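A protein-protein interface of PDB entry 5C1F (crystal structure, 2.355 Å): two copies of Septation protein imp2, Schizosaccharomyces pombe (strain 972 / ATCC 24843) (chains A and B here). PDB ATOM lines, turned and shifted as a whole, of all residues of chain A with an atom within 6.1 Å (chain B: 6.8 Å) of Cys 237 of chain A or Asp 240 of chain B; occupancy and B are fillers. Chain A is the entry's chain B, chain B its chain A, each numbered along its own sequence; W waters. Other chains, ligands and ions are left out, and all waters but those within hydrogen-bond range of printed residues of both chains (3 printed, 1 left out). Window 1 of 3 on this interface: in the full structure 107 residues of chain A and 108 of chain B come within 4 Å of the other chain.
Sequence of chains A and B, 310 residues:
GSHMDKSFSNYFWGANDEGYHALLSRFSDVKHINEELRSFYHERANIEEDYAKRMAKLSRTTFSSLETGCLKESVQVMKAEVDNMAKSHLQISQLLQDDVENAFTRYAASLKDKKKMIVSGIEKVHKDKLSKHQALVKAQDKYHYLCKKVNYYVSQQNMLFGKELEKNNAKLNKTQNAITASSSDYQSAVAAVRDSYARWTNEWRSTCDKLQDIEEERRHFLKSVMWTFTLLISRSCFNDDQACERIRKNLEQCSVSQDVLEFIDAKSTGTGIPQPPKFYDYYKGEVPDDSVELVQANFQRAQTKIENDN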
ATOM      1  N   ARG A  44     -24.527  -4.285 -30.046  1.00  0.00           N
ATOM      2  CA  ARG A  44     -23.738  -5.229 -29.263  1.00  0.00           C
ATOM      3  C   ARG A  44     -23.543  -6.544 -30.014  1.00  0.00           C
ATOM      4  O   ARG A  44     -22.449  -7.111 -30.018  1.00  0.00           O
ATOM      5  CB  ARG A  44     -24.397  -5.490 -27.908  1.00  0.00           C
ATOM      6  CG  ARG A  44     -23.612  -6.435 -27.012  1.00  0.00           C
ATOM      7  CD  ARG A  44     -22.180  -5.953 -26.807  1.00  0.00           C
ATOM      8  NE  ARG A  44     -21.412  -6.880 -25.981  1.00  0.00           N
ATOM      9  CZ  ARG A  44     -20.748  -7.930 -26.455  1.00  0.00           C
ATOM     10  NH1 ARG A  44     -20.751  -8.190 -27.756  1.00  0.00           N
ATOM     11  NH2 ARG A  44     -20.077  -8.723 -25.627  1.00  0.00           N
ATOM     12  N   LEU A 232     -25.509 -15.448 -22.327  1.00  0.00           N
ATOM     13  CA  LEU A 232     -24.820 -15.588 -23.604  1.00  0.00           C
ATOM     14  C   LEU A 232     -23.370 -15.115 -23.522  1.00  0.00           C
ATOM     15  O   LEU A 232     -22.472 -15.758 -24.067  1.00  0.00           O
ATOM     16  CB  LEU A 232     -25.566 -14.819 -24.700  1.00  0.00           C
ATOM     17  CG  LEU A 232     -26.812 -15.531 -25.235  1.00  0.00           C
ATOM     18  CD1 LEU A 232     -27.528 -14.690 -26.286  1.00  0.00           C
ATOM     19  CD2 LEU A 232     -26.430 -16.886 -25.804  1.00  0.00           C
ATOM     20  N   ILE A 233     -23.138 -13.999 -22.841  1.00  0.00           N
ATOM     21  CA  ILE A 233     -21.780 -13.487 -22.700  1.00  0.00           C
ATOM     22  C   ILE A 233     -20.965 -14.404 -21.792  1.00  0.00           C
ATOM     23  O   ILE A 233     -19.810 -14.709 -22.090  1.00  0.00           O
ATOM     24  CB  ILE A 233     -21.761 -12.050 -22.151  1.00  0.00           C
ATOM     25  CG1 ILE A 233     -22.553 -11.123 -23.071  1.00  0.00           C
ATOM     26  CG2 ILE A 233     -20.330 -11.544 -22.022  1.00  0.00           C
ATOM     27  CD1 ILE A 233     -22.093 -11.175 -24.511  1.00  0.00           C
ATOM     28  N   SER A 234     -21.571 -14.854 -20.696  1.00  0.00           N
ATOM     29  CA  SER A 234     -20.919 -15.808 -19.800  1.00  0.00           C
ATOM     30  C   SER A 234     -20.563 -17.100 -20.532  1.00  0.00           C
ATOM     31  O   SER A 234     -19.492 -17.663 -20.322  1.00  0.00           O
ATOM     32  CB  SER A 234     -21.811 -16.124 -18.598  1.00  0.00           C
ATOM     33  OG  SER A 234     -21.864 -15.032 -17.701  1.00  0.00           O
ATOM     34  N   ARG A 235     -21.464 -17.563 -21.393  1.00  0.00           N
ATOM     35  CA  ARG A 235     -21.218 -18.766 -22.182  1.00  0.00           C
ATOM     36  C   ARG A 235     -20.017 -18.559 -23.103  1.00  0.00           C
ATOM     37  O   ARG A 235     -19.191 -19.455 -23.281  1.00  0.00           O
ATOM     38  CB  ARG A 235     -22.462 -19.143 -22.991  1.00  0.00           C
ATOM     39  CG  ARG A 235     -22.286 -20.377 -23.863  1.00  0.00           C
ATOM     40  CD  ARG A 235     -23.602 -20.781 -24.512  1.00  0.00           C
ATOM     41  NE  ARG A 235     -24.586 -21.217 -23.525  1.00  0.00           N
ATOM     42  CZ  ARG A 235     -24.876 -22.489 -23.275  1.00  0.00           C
ATOM     43  NH1 ARG A 235     -24.265 -23.457 -23.947  1.00  0.00           N
ATOM     44  NH2 ARG A 235     -25.784 -22.793 -22.356  1.00  0.00           N
ATOM     45  N   SER A 236     -19.928 -17.362 -23.675  1.00  0.00           N
ATOM     46  CA  SER A 236     -18.795 -16.973 -24.506  1.00  0.00           C
ATOM     47  C   SER A 236     -17.492 -17.019 -23.716  1.00  0.00           C
ATOM     48  O   SER A 236     -16.471 -17.499 -24.211  1.00  0.00           O
ATOM     49  CB  SER A 236     -19.018 -15.570 -25.078  1.00  0.00           C
ATOM     50  OG  SER A 236     -17.908 -15.142 -25.845  1.00  0.00           O
ATOM     51  N   CYS A 237     -17.532 -16.509 -22.488  1.00  0.00           N
ATOM     52  CA  CYS A 237     -16.376 -16.542 -21.599  1.00  0.00           C
ATOM     53  C   CYS A 237     -15.948 -17.969 -21.321  1.00  0.00           C
ATOM     54  O   CYS A 237     -14.757 -18.287 -21.323  1.00  0.00           O
ATOM     55  CB  CYS A 237     -16.687 -15.836 -20.280  1.00  0.00           C
ATOM     56  SG  CYS A 237     -17.020 -14.077 -20.446  1.00  0.00           S
ATOM     57  N   PHE A 238     -16.930 -18.827 -21.076  1.00  0.00           N
ATOM     58  CA  PHE A 238     -16.656 -20.220 -20.780  1.00  0.00           C
ATOM     59  C   PHE A 238     -15.924 -20.919 -21.933  1.00  0.00           C
ATOM     60  O   PHE A 238     -14.898 -21.566 -21.715  1.00  0.00           O
ATOM     61  CB  PHE A 238     -17.956 -20.956 -20.450  1.00  0.00           C
ATOM     62  CG  PHE A 238     -17.760 -22.408 -20.118  1.00  0.00           C
ATOM     63  CD1 PHE A 238     -17.315 -22.789 -18.861  1.00  0.00           C
ATOM     64  CD2 PHE A 238     -18.010 -23.392 -21.063  1.00  0.00           C
ATOM     65  CE1 PHE A 238     -17.125 -24.128 -18.549  1.00  0.00           C
ATOM     66  CE2 PHE A 238     -17.823 -24.733 -20.756  1.00  0.00           C
ATOM     67  CZ  PHE A 238     -17.380 -25.100 -19.498  1.00  0.00           C
ATOM     68  N   ASN A 239     -16.461 -20.777 -23.145  1.00  0.00           N
ATOM     69  CA  ASN A 239     -15.894 -21.412 -24.334  1.00  0.00           C
ATOM     70  C   ASN A 239     -14.457 -20.983 -24.614  1.00  0.00           C
ATOM     71  O   ASN A 239     -13.607 -21.810 -24.940  1.00  0.00           O
ATOM     72  CB  ASN A 239     -16.754 -21.108 -25.562  1.00  0.00           C
ATOM     73  CG  ASN A 239     -18.166 -21.652 -25.443  1.00  0.00           C
ATOM     74  OD1 ASN A 239     -18.416 -22.625 -24.731  1.00  0.00           O
ATOM     75  ND2 ASN A 239     -19.099 -21.026 -26.152  1.00  0.00           N
ATOM     76  N   ASP A 240     -14.199 -19.686 -24.494  1.00  0.00           N
ATOM     77  CA  ASP A 240     -12.872 -19.138 -24.754  1.00  0.00           C
ATOM     78  C   ASP A 240     -11.875 -19.626 -23.706  1.00  0.00           C
ATOM     79  O   ASP A 240     -10.727 -19.943 -24.024  1.00  0.00           O
ATOM     80  CB  ASP A 240     -12.907 -17.609 -24.783  1.00  0.00           C
ATOM     81  CG  ASP A 240     -13.350 -17.062 -26.125  1.00  0.00           C
ATOM     82  OD1 ASP A 240     -13.993 -17.809 -26.889  1.00  0.00           O
ATOM     83  OD2 ASP A 240     -13.053 -15.885 -26.418  1.00  0.00           O
ATOM     84  N   ASP A 241     -12.325 -19.697 -22.458  1.00  0.00           N
ATOM     85  CA  ASP A 241     -11.466 -20.159 -21.376  1.00  0.00           C
ATOM     86  C   ASP A 241     -11.106 -21.625 -21.565  1.00  0.00           C
ATOM     87  O   ASP A 241      -9.965 -22.021 -21.340  1.00  0.00           O
ATOM     88  CB  ASP A 241     -12.139 -19.952 -20.018  1.00  0.00           C
ATOM     89  CG  ASP A 241     -11.212 -20.258 -18.863  1.00  0.00           C
ATOM     90  OD1 ASP A 241     -10.096 -19.697 -18.830  1.00  0.00           O
ATOM     91  OD2 ASP A 241     -11.593 -21.069 -17.994  1.00  0.00           O
ATOM     92  N   GLN A 242     -12.082 -22.425 -21.984  1.00  0.00           N
ATOM     93  CA  GLN A 242     -11.841 -23.833 -22.276  1.00  0.00           C
ATOM     94  C   GLN A 242     -10.828 -23.975 -23.404  1.00  0.00           C
ATOM     95  O   GLN A 242      -9.944 -24.830 -23.351  1.00  0.00           O
ATOM     96  CB  GLN A 242     -13.143 -24.550 -22.644  1.00  0.00           C
ATOM     97  CG  GLN A 242     -14.135 -24.680 -21.495  1.00  0.00           C
ATOM     98  CD  GLN A 242     -13.582 -25.471 -20.323  1.00  0.00           C
ATOM     99  OE1 GLN A 242     -13.279 -24.910 -19.268  1.00  0.00           O
ATOM    100  NE2 GLN A 242     -13.456 -26.782 -20.500  1.00  0.00           N
ATOM    101  N   TYR B  51     -12.448  -4.118 -30.888  1.00  0.00           N
ATOM    102  CA  TYR B  51     -13.528  -4.695 -30.098  1.00  0.00           C
ATOM    103  C   TYR B  51     -13.780  -3.851 -28.844  1.00  0.00           C
ATOM    104  O   TYR B  51     -14.912  -3.448 -28.564  1.00  0.00           O
ATOM    105  CB  TYR B  51     -13.160  -6.138 -29.736  1.00  0.00           C
ATOM    106  CG  TYR B  51     -14.230  -6.983 -29.078  1.00  0.00           C
ATOM    107  CD1 TYR B  51     -15.481  -7.154 -29.658  1.00  0.00           C
ATOM    108  CD2 TYR B  51     -13.960  -7.669 -27.901  1.00  0.00           C
ATOM    109  CE1 TYR B  51     -16.447  -7.956 -29.055  1.00  0.00           C
ATOM    110  CE2 TYR B  51     -14.912  -8.471 -27.297  1.00  0.00           C
ATOM    111  CZ  TYR B  51     -16.152  -8.613 -27.874  1.00  0.00           C
ATOM    112  OH  TYR B  51     -17.095  -9.413 -27.263  1.00  0.00           O
ATOM    113  N   MET B  55     -17.014  -1.343 -28.060  1.00  0.00           N
ATOM    114  CA  MET B  55     -17.805  -1.666 -26.879  1.00  0.00           C
ATOM    115  C   MET B  55     -17.911  -0.460 -25.949  1.00  0.00           C
ATOM    116  O   MET B  55     -18.951  -0.239 -25.321  1.00  0.00           O
ATOM    117  CB  MET B  55     -17.204  -2.859 -26.138  1.00  0.00           C
ATOM    118  CG  MET B  55     -18.130  -3.453 -25.091  1.00  0.00           C
ATOM    119  SD  MET B  55     -17.456  -4.953 -24.361  1.00  0.00           S
ATOM    120  CE  MET B  55     -17.238  -5.966 -25.819  1.00  0.00           C
ATOM    121  N   GLU B  81     -21.777  -2.048 -16.680  1.00  0.00           N
ATOM    122  CA  GLU B  81     -21.008  -3.285 -16.665  1.00  0.00           C
ATOM    123  C   GLU B  81     -20.509  -3.653 -18.058  1.00  0.00           C
ATOM    124  O   GLU B  81     -19.470  -4.299 -18.197  1.00  0.00           O
ATOM    125  CB  GLU B  81     -21.825  -4.434 -16.063  1.00  0.00           C
ATOM    126  CG  GLU B  81     -22.037  -4.324 -14.549  1.00  0.00           C
ATOM    127  CD  GLU B  81     -20.733  -4.307 -13.747  1.00  0.00           C
ATOM    128  OE1 GLU B  81     -19.661  -4.625 -14.307  1.00  0.00           O
ATOM    129  OE2 GLU B  81     -20.781  -3.974 -12.542  1.00  0.00           O
ATOM    130  N   ASN B  84     -17.512  -1.680 -18.144  1.00  0.00           N
ATOM    131  CA  ASN B  84     -16.442  -2.364 -17.421  1.00  0.00           C
ATOM    132  C   ASN B  84     -15.811  -3.459 -18.271  1.00  0.00           C
ATOM    133  O   ASN B  84     -14.611  -3.713 -18.193  1.00  0.00           O
ATOM    134  CB  ASN B  84     -16.962  -2.953 -16.110  1.00  0.00           C
ATOM    135  CG  ASN B  84     -17.111  -1.910 -15.026  1.00  0.00           C
ATOM    136  OD1 ASN B  84     -16.424  -0.885 -15.039  1.00  0.00           O
ATOM    137  ND2 ASN B  84     -18.006  -2.163 -14.077  1.00  0.00           N
ATOM    138  N   MET B  85     -16.629  -4.105 -19.088  1.00  0.00           N
ATOM    139  CA  MET B  85     -16.122  -5.117 -19.996  1.00  0.00           C
ATOM    140  C   MET B  85     -15.258  -4.471 -21.079  1.00  0.00           C
ATOM    141  O   MET B  85     -14.220  -5.013 -21.455  1.00  0.00           O
ATOM    142  CB  MET B  85     -17.276  -5.911 -20.608  1.00  0.00           C
ATOM    143  CG  MET B  85     -17.929  -6.874 -19.621  1.00  0.00           C
ATOM    144  SD  MET B  85     -19.213  -7.907 -20.356  1.00  0.00           S
ATOM    145  CE  MET B  85     -20.677  -7.237 -19.582  1.00  0.00           C
ATOM    146  N   ALA B  86     -15.676  -3.303 -21.556  1.00  0.00           N
ATOM    147  CA  ALA B  86     -14.897  -2.544 -22.531  1.00  0.00           C
ATOM    148  C   ALA B  86     -13.525  -2.163 -21.977  1.00  0.00           C
ATOM    149  O   ALA B  86     -12.507  -2.367 -22.635  1.00  0.00           O
ATOM    150  CB  ALA B  86     -15.656  -1.293 -22.965  1.00  0.00           C
ATOM    151  N   SER B  88     -11.850  -3.535 -19.602  1.00  0.00           N
ATOM    152  CA  SER B  88     -11.054  -4.741 -19.449  1.00  0.00           C
ATOM    153  C   SER B  88     -10.453  -5.147 -20.790  1.00  0.00           C
ATOM    154  O   SER B  88      -9.247  -5.364 -20.896  1.00  0.00           O
ATOM    155  CB  SER B  88     -11.903  -5.877 -18.872  1.00  0.00           C
ATOM    156  OG  SER B  88     -11.191  -7.104 -18.863  1.00  0.00           O
ATOM    157  N   HIS B  89     -11.299  -5.236 -21.812  1.00  0.00           N
ATOM    158  CA  HIS B  89     -10.836  -5.611 -23.143  1.00  0.00           C
ATOM    159  C   HIS B  89      -9.797  -4.625 -23.686  1.00  0.00           C
ATOM    160  O   HIS B  89      -8.884  -5.028 -24.405  1.00  0.00           O
ATOM    161  CB  HIS B  89     -12.021  -5.731 -24.105  1.00  0.00           C
ATOM    162  CG  HIS B  89     -12.786  -7.008 -23.957  1.00  0.00           C
ATOM    163  ND1 HIS B  89     -12.341  -8.205 -24.480  1.00  0.00           N
ATOM    164  CD2 HIS B  89     -13.959  -7.283 -23.341  1.00  0.00           C
ATOM    165  CE1 HIS B  89     -13.209  -9.158 -24.194  1.00  0.00           C
ATOM    166  NE2 HIS B  89     -14.200  -8.626 -23.501  1.00  0.00           N
ATOM    167  N   ILE B 233      -6.170 -14.051 -22.218  1.00  0.00           N
ATOM    168  CA  ILE B 233      -7.532 -14.299 -22.691  1.00  0.00           C
ATOM    169  C   ILE B 233      -8.405 -14.882 -21.579  1.00  0.00           C
ATOM    170  O   ILE B 233      -9.574 -14.518 -21.438  1.00  0.00           O
ATOM    171  CB  ILE B 233      -7.558 -15.253 -23.911  1.00  0.00           C
ATOM    172  CG1 ILE B 233      -6.733 -14.684 -25.067  1.00  0.00           C
ATOM    173  CG2 ILE B 233      -8.984 -15.495 -24.368  1.00  0.00           C
ATOM    174  CD1 ILE B 233      -7.270 -13.384 -25.627  1.00  0.00           C
ATOM    175  N   SER B 234      -7.839 -15.790 -20.792  1.00  0.00           N
ATOM    176  CA  SER B 234      -8.563 -16.358 -19.660  1.00  0.00           C
ATOM    177  C   SER B 234      -8.917 -15.274 -18.641  1.00  0.00           C
ATOM    178  O   SER B 234      -9.982 -15.319 -18.028  1.00  0.00           O
ATOM    179  CB  SER B 234      -7.747 -17.466 -18.990  1.00  0.00           C
ATOM    180  OG  SER B 234      -7.699 -18.630 -19.796  1.00  0.00           O
ATOM    181  N   ARG B 235      -8.021 -14.303 -18.469  1.00  0.00           N
ATOM    182  CA  ARG B 235      -8.272 -13.172 -17.578  1.00  0.00           C
ATOM    183  C   ARG B 235      -9.433 -12.340 -18.111  1.00  0.00           C
ATOM    184  O   ARG B 235     -10.281 -11.874 -17.352  1.00  0.00           O
ATOM    185  CB  ARG B 235      -7.016 -12.306 -17.432  1.00  0.00           C
ATOM    186  CG  ARG B 235      -7.194 -11.067 -16.561  1.00  0.00           C
ATOM    187  CD  ARG B 235      -7.498 -11.424 -15.104  1.00  0.00           C
ATOM    188  NE  ARG B 235      -7.622 -10.234 -14.261  1.00  0.00           N
ATOM    189  CZ  ARG B 235      -8.018 -10.250 -12.990  1.00  0.00           C
ATOM    190  NH1 ARG B 235      -8.337 -11.395 -12.402  1.00  0.00           N
ATOM    191  NH2 ARG B 235      -8.097  -9.117 -12.302  1.00  0.00           N
ATOM    192  N   SER B 236      -9.458 -12.167 -19.428  1.00  0.00           N
ATOM    193  CA  SER B 236     -10.534 -11.450 -20.097  1.00  0.00           C
ATOM    194  C   SER B 236     -11.870 -12.139 -19.849  1.00  0.00           C
ATOM    195  O   SER B 236     -12.893 -11.483 -19.642  1.00  0.00           O
ATOM    196  CB  SER B 236     -10.256 -11.355 -21.599  1.00  0.00           C
ATOM    197  OG  SER B 236     -11.311 -10.697 -22.274  1.00  0.00           O
ATOM    198  N   CYS B 237     -11.849 -13.467 -19.868  1.00  0.00           N
ATOM    199  CA  CYS B 237     -13.055 -14.250 -19.649  1.00  0.00           C
ATOM    200  C   CYS B 237     -13.540 -14.123 -18.211  1.00  0.00           C
ATOM    201  O   CYS B 237     -14.727 -13.933 -17.963  1.00  0.00           O
ATOM    202  CB  CYS B 237     -12.807 -15.714 -20.001  1.00  0.00           C
ATOM    203  SG  CYS B 237     -12.438 -15.979 -21.747  1.00  0.00           S
ATOM    204  N   PHE B 238     -12.612 -14.226 -17.266  1.00  0.00           N
ATOM    205  CA  PHE B 238     -12.940 -14.052 -15.856  1.00  0.00           C
ATOM    206  C   PHE B 238     -13.578 -12.682 -15.607  1.00  0.00           C
ATOM    207  O   PHE B 238     -14.653 -12.587 -15.012  1.00  0.00           O
ATOM    208  CB  PHE B 238     -11.680 -14.224 -14.999  1.00  0.00           C
ATOM    209  CG  PHE B 238     -11.912 -14.029 -13.527  1.00  0.00           C
ATOM    210  CD1 PHE B 238     -12.400 -15.063 -12.748  1.00  0.00           C
ATOM    211  CD2 PHE B 238     -11.628 -12.812 -12.916  1.00  0.00           C
ATOM    212  CE1 PHE B 238     -12.609 -14.889 -11.387  1.00  0.00           C
ATOM    213  CE2 PHE B 238     -11.837 -12.633 -11.557  1.00  0.00           C
ATOM    214  CZ  PHE B 238     -12.327 -13.672 -10.792  1.00  0.00           C
ATOM    215  N   ASN B 239     -12.919 -11.628 -16.082  1.00  0.00           N
ATOM    216  CA  ASN B 239     -13.412 -10.263 -15.902  1.00  0.00           C
ATOM    217  C   ASN B 239     -14.826 -10.062 -16.446  1.00  0.00           C
ATOM    218  O   ASN B 239     -15.695  -9.538 -15.748  1.00  0.00           O
ATOM    219  CB  ASN B 239     -12.464  -9.261 -16.562  1.00  0.00           C
ATOM    220  CG  ASN B 239     -11.139  -9.142 -15.834  1.00  0.00           C
ATOM    221  OD1 ASN B 239     -10.991  -9.612 -14.703  1.00  0.00           O
ATOM    222  ND2 ASN B 239     -10.169  -8.499 -16.477  1.00  0.00           N
ATOM    223  N   ASP B 240     -15.051 -10.474 -17.691  1.00  0.00           N
ATOM    224  CA  ASP B 240     -16.358 -10.317 -18.318  1.00  0.00           C
ATOM    225  C   ASP B 240     -17.422 -11.142 -17.604  1.00  0.00           C
ATOM    226  O   ASP B 240     -18.557 -10.693 -17.440  1.00  0.00           O
ATOM    227  CB  ASP B 240     -16.300 -10.705 -19.795  1.00  0.00           C
ATOM    228  CG  ASP B 240     -15.670  -9.630 -20.656  1.00  0.00           C
ATOM    229  OD1 ASP B 240     -15.051  -8.701 -20.095  1.00  0.00           O
ATOM    230  OD2 ASP B 240     -15.790  -9.720 -21.896  1.00  0.00           O
ATOM    231  N   ASP B 241     -17.056 -12.346 -17.178  1.00  0.00           N
ATOM    232  CA  ASP B 241     -18.002 -13.201 -16.474  1.00  0.00           C
ATOM    233  C   ASP B 241     -18.384 -12.606 -15.120  1.00  0.00           C
ATOM    234  O   ASP B 241     -19.530 -12.737 -14.682  1.00  0.00           O
ATOM    235  CB  ASP B 241     -17.437 -14.608 -16.282  1.00  0.00           C
ATOM    236  CG  ASP B 241     -18.415 -15.527 -15.584  1.00  0.00           C
ATOM    237  OD1 ASP B 241     -19.575 -15.603 -16.040  1.00  0.00           O
ATOM    238  OD2 ASP B 241     -18.039 -16.146 -14.568  1.00  0.00           O
ATOM    239  N   GLN B 242     -17.426 -11.956 -14.459  1.00  0.00           N
ATOM    240  CA  GLN B 242     -17.708 -11.296 -13.187  1.00  0.00           C
ATOM    241  C   GLN B 242     -18.659 -10.124 -13.396  1.00  0.00           C
ATOM    242  O   GLN B 242     -19.534  -9.873 -12.568  1.00  0.00           O
ATOM    243  CB  GLN B 242     -16.421 -10.813 -12.512  1.00  0.00           C
ATOM    244  CG  GLN B 242     -15.545 -11.922 -11.951  1.00  0.00           C
ATOM    245  CD  GLN B 242     -16.239 -12.734 -10.873  1.00  0.00           C
ATOM    246  OE1 GLN B 242     -16.462 -12.251  -9.762  1.00  0.00           O
ATOM    247  NE2 GLN B 242     -16.582 -13.975 -11.195  1.00  0.00           N
ATOM    248  N   ALA B 243     -18.490  -9.416 -14.510  1.00  0.00           N
ATOM    249  CA  ALA B 243     -19.367  -8.297 -14.840  1.00  0.00           C
ATOM    250  C   ALA B 243     -20.790  -8.782 -15.114  1.00  0.00           C
ATOM    251  O   ALA B 243     -21.763  -8.153 -14.688  1.00  0.00           O
ATOM    252  CB  ALA B 243     -18.825  -7.531 -16.039  1.00  0.00           C
ATOM    253  N   CYS B 244     -20.902  -9.901 -15.825  1.00  0.00           N
ATOM    254  CA  CYS B 244     -22.199 -10.503 -16.109  1.00  0.00           C
ATOM    255  C   CYS B 244     -22.894 -10.928 -14.830  1.00  0.00           C
ATOM    256  O   CYS B 244     -24.103 -10.765 -14.690  1.00  0.00           O
ATOM    257  CB  CYS B 244     -22.048 -11.708 -17.035  1.00  0.00           C
ATOM    258  SG  CYS B 244     -21.582 -11.270 -18.710  1.00  0.00           S
ATOM    259  N   GLU B 245     -22.115 -11.476 -13.902  1.00  0.00           N
ATOM    260  CA  GLU B 245     -22.658 -11.959 -12.644  1.00  0.00           C
ATOM    261  C   GLU B 245     -23.226 -10.799 -11.838  1.00  0.00           C
ATOM    262  O   GLU B 245     -24.260 -10.933 -11.186  1.00  0.00           O
ATOM    263  CB  GLU B 245     -21.586 -12.697 -11.842  1.00  0.00           C
ATOM    264  CG  GLU B 245     -22.153 -13.624 -10.779  1.00  0.00           C
ATOM    265  CD  GLU B 245     -22.874 -14.820 -11.372  1.00  0.00           C
ATOM    266  OE1 GLU B 245     -22.234 -15.592 -12.122  1.00  0.00           O
ATOM    267  OE2 GLU B 245     -24.080 -14.989 -11.094  1.00  0.00           O
ATOM    268  N   ARG B 246     -22.556  -9.652 -11.897  1.00  0.00           N
ATOM    269  CA  ARG B 246     -23.032  -8.471 -11.183  1.00  0.00           C
ATOM    270  C   ARG B 246     -24.342  -7.953 -11.786  1.00  0.00           C
ATOM    271  O   ARG B 246     -25.211  -7.465 -11.061  1.00  0.00           O
ATOM    272  CB  ARG B 246     -21.961  -7.376 -11.175  1.00  0.00           C
ATOM    273  CG  ARG B 246     -20.754  -7.718 -10.298  1.00  0.00           C
ATOM    274  CD  ARG B 246     -19.817  -6.527 -10.073  1.00  0.00           C
ATOM    275  NE  ARG B 246     -19.164  -6.076 -11.299  1.00  0.00           N
ATOM    276  CZ  ARG B 246     -18.010  -6.554 -11.757  1.00  0.00           C
ATOM    277  NH1 ARG B 246     -17.375  -7.512 -11.094  1.00  0.00           N
ATOM    278  NH2 ARG B 246     -17.495  -6.078 -12.883  1.00  0.00           N
HETATM  279  O   HOH W   1     -19.931  -6.721 -23.343  1.00  0.00           O
HETATM  280  O   HOH W   2     -18.411 -12.217 -25.759  1.00  0.00           O
HETATM  281  O   HOH W   3     -17.816  -8.971 -23.786  1.00  0.00           O
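SG of Cys 237 of chain A is in hydrogen-bond range of N of Asp 241 of chain B, at 3.7 Å. The side-chain sulfur (SG) of Cys 237 of chain B lies within hydrogen-bond range of the backbone NH (N) of Asp 241 of chain A, 3.8 Å away. The guanidinium group of Arg 44 of chain A lies within hydrogen-bond range of the side-chain hydroxyl of Tyr 51 of chain B, at 3.5 Å. The side-chain carboxylate (OD1) of Asp 241 of chain B sits at hydrogen-bond distance from the side-chain hydroxyl (OG) of Ser 234 of chain A (2.9 Å). The side-chain carboxylate of Asp 241 of chain A lies within hydrogen-bond range of the side-chain hydroxyl of Ser 234 of chain B (2.8 Å). The backbone carbonyl oxygen (O) of Cys 237 of chain A is in hydrogen-bond range of the side-chain sulfur (SG) of Cys 237 of chain B (3.3 Å).
The backbone carbonyl oxygen of Ile 233 of chain A lies within hydrogen-bond range of the side-chain sulfur of Cys 237 of chain A (3.3 Å). The backbone carbonyl oxygen (O) of Asp 240 of chain B sits at hydrogen-bond distance from the side-chain sulfur (SG) of Cys 244 of chain B, 3.3 Å away. SG of Cys 237 of chain B lies within hydrogen-bond range of O of Ile 233 of chain B, 3.2 Å away. SD of Met 55 of chain B lies within hydrogen-bond range of N of Ala 86 of chain B, at 3.7 Å. OD2 of Asp 240 of chain B is in hydrogen-bond range of NE2 of His 89 of chain B.
Among the printed residues, pairs that only touch across the chains: Arg 44 of chain A with Met 55 of chain B (3.96 Å), Ile 233 of chain A with Cys 244 of chain B (3.5 Å), Ser 234 of chain A with Cys 244 of chain B (3.4 Å), Cys 237 of chain A with Asp 240 of chain B (3.5 Å) and Asp 240 of chain A with Cys 237 of chain B (3.5 Å).
Of chain B, only Cys 237 (3.3 Å), Asp 240 (3.5 Å) and Asp 241 (3.7 Å) come within 4 Å of Cys 237 of chain A. Asp 240 of chain B touches just one residue of chain A: Cys 237. Of the printed residues of chain A, Cys 244 of chain B touches Ile 233 (3.5 Å) and Ser 234 (3.4 Å). Of the printed residues of chain A, Met 55 of chain B touches Arg 44. His 89 of chain B touches none of the printed residues of chain A. The nearest residue of chain A that does not touch Asp 240 of chain B is Ile 233 of chain A (4.7 Å). The nearest printed residue of chain A that does not touch Tyr 51 of chain B is Ser 236 of chain A (6.0 Å).
Printed residues of chain B that touch a printed residue of chain A: Tyr 51, Met 55, Ser 234, Cys 237, Asp 240, Asp 241 and Cys 244. Hydrophobic or aromatic side chains of chain B within 4 Å of the printed part of chain A: Tyr 51 and Met 55. Of the 12 printed residues of chain A, 6 touch a printed residue of chain B. Printed residues of chain A that touch a printed residue of chain B: Arg 44, Ile 233, Ser 234, Cys 237, Asp 240 and Asp 241. Among the printed residues, no Asp or Glu carboxylate lies within 4 Å of a Lys or Arg side-chain nitrogen of the other chain.
Ser 234 of chain A touches Asp 241 of chain B, and with the chains exchanged Asp 241 of chain A touches Ser 234 of chain B. Cys 237 of chain B touches its own counterpart, Cys 237 of chain A. Cys 237 of chain A touches Asp 240 of chain B, and with the chains exchanged Asp 240 of chain A touches Cys 237 of chain B. Cys 237 of chain A touches Asp 241 of chain B, and with the chains exchanged Asp 241 of chain A touches Cys 237 of chain B. Positions printed for both chains: 233, 234, 235, 236, 237, 238, 239, 240, 241 and 242.
Water W3 lies within hydrogen-bond range of the side-chain carboxylate (OD2) of Asp 240 of chain B (2.9 Å) and the guanidinium group (NH2) of Arg 44 of chain A (2.9 Å). Water W2 bridges OG of Ser 236 of chain A (3.0 Å) and OH of Tyr 51 of chain B (3.4 Å). Water W1 lies within hydrogen-bond range of the guanidinium group (NE) of Arg 44 of chain A (3.0 Å), the side-chain sulfur (SD) of Met 55 of chain B (3.2 Å) and the side-chain sulfur (SD) of Met 85 of chain B (3.3 Å).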
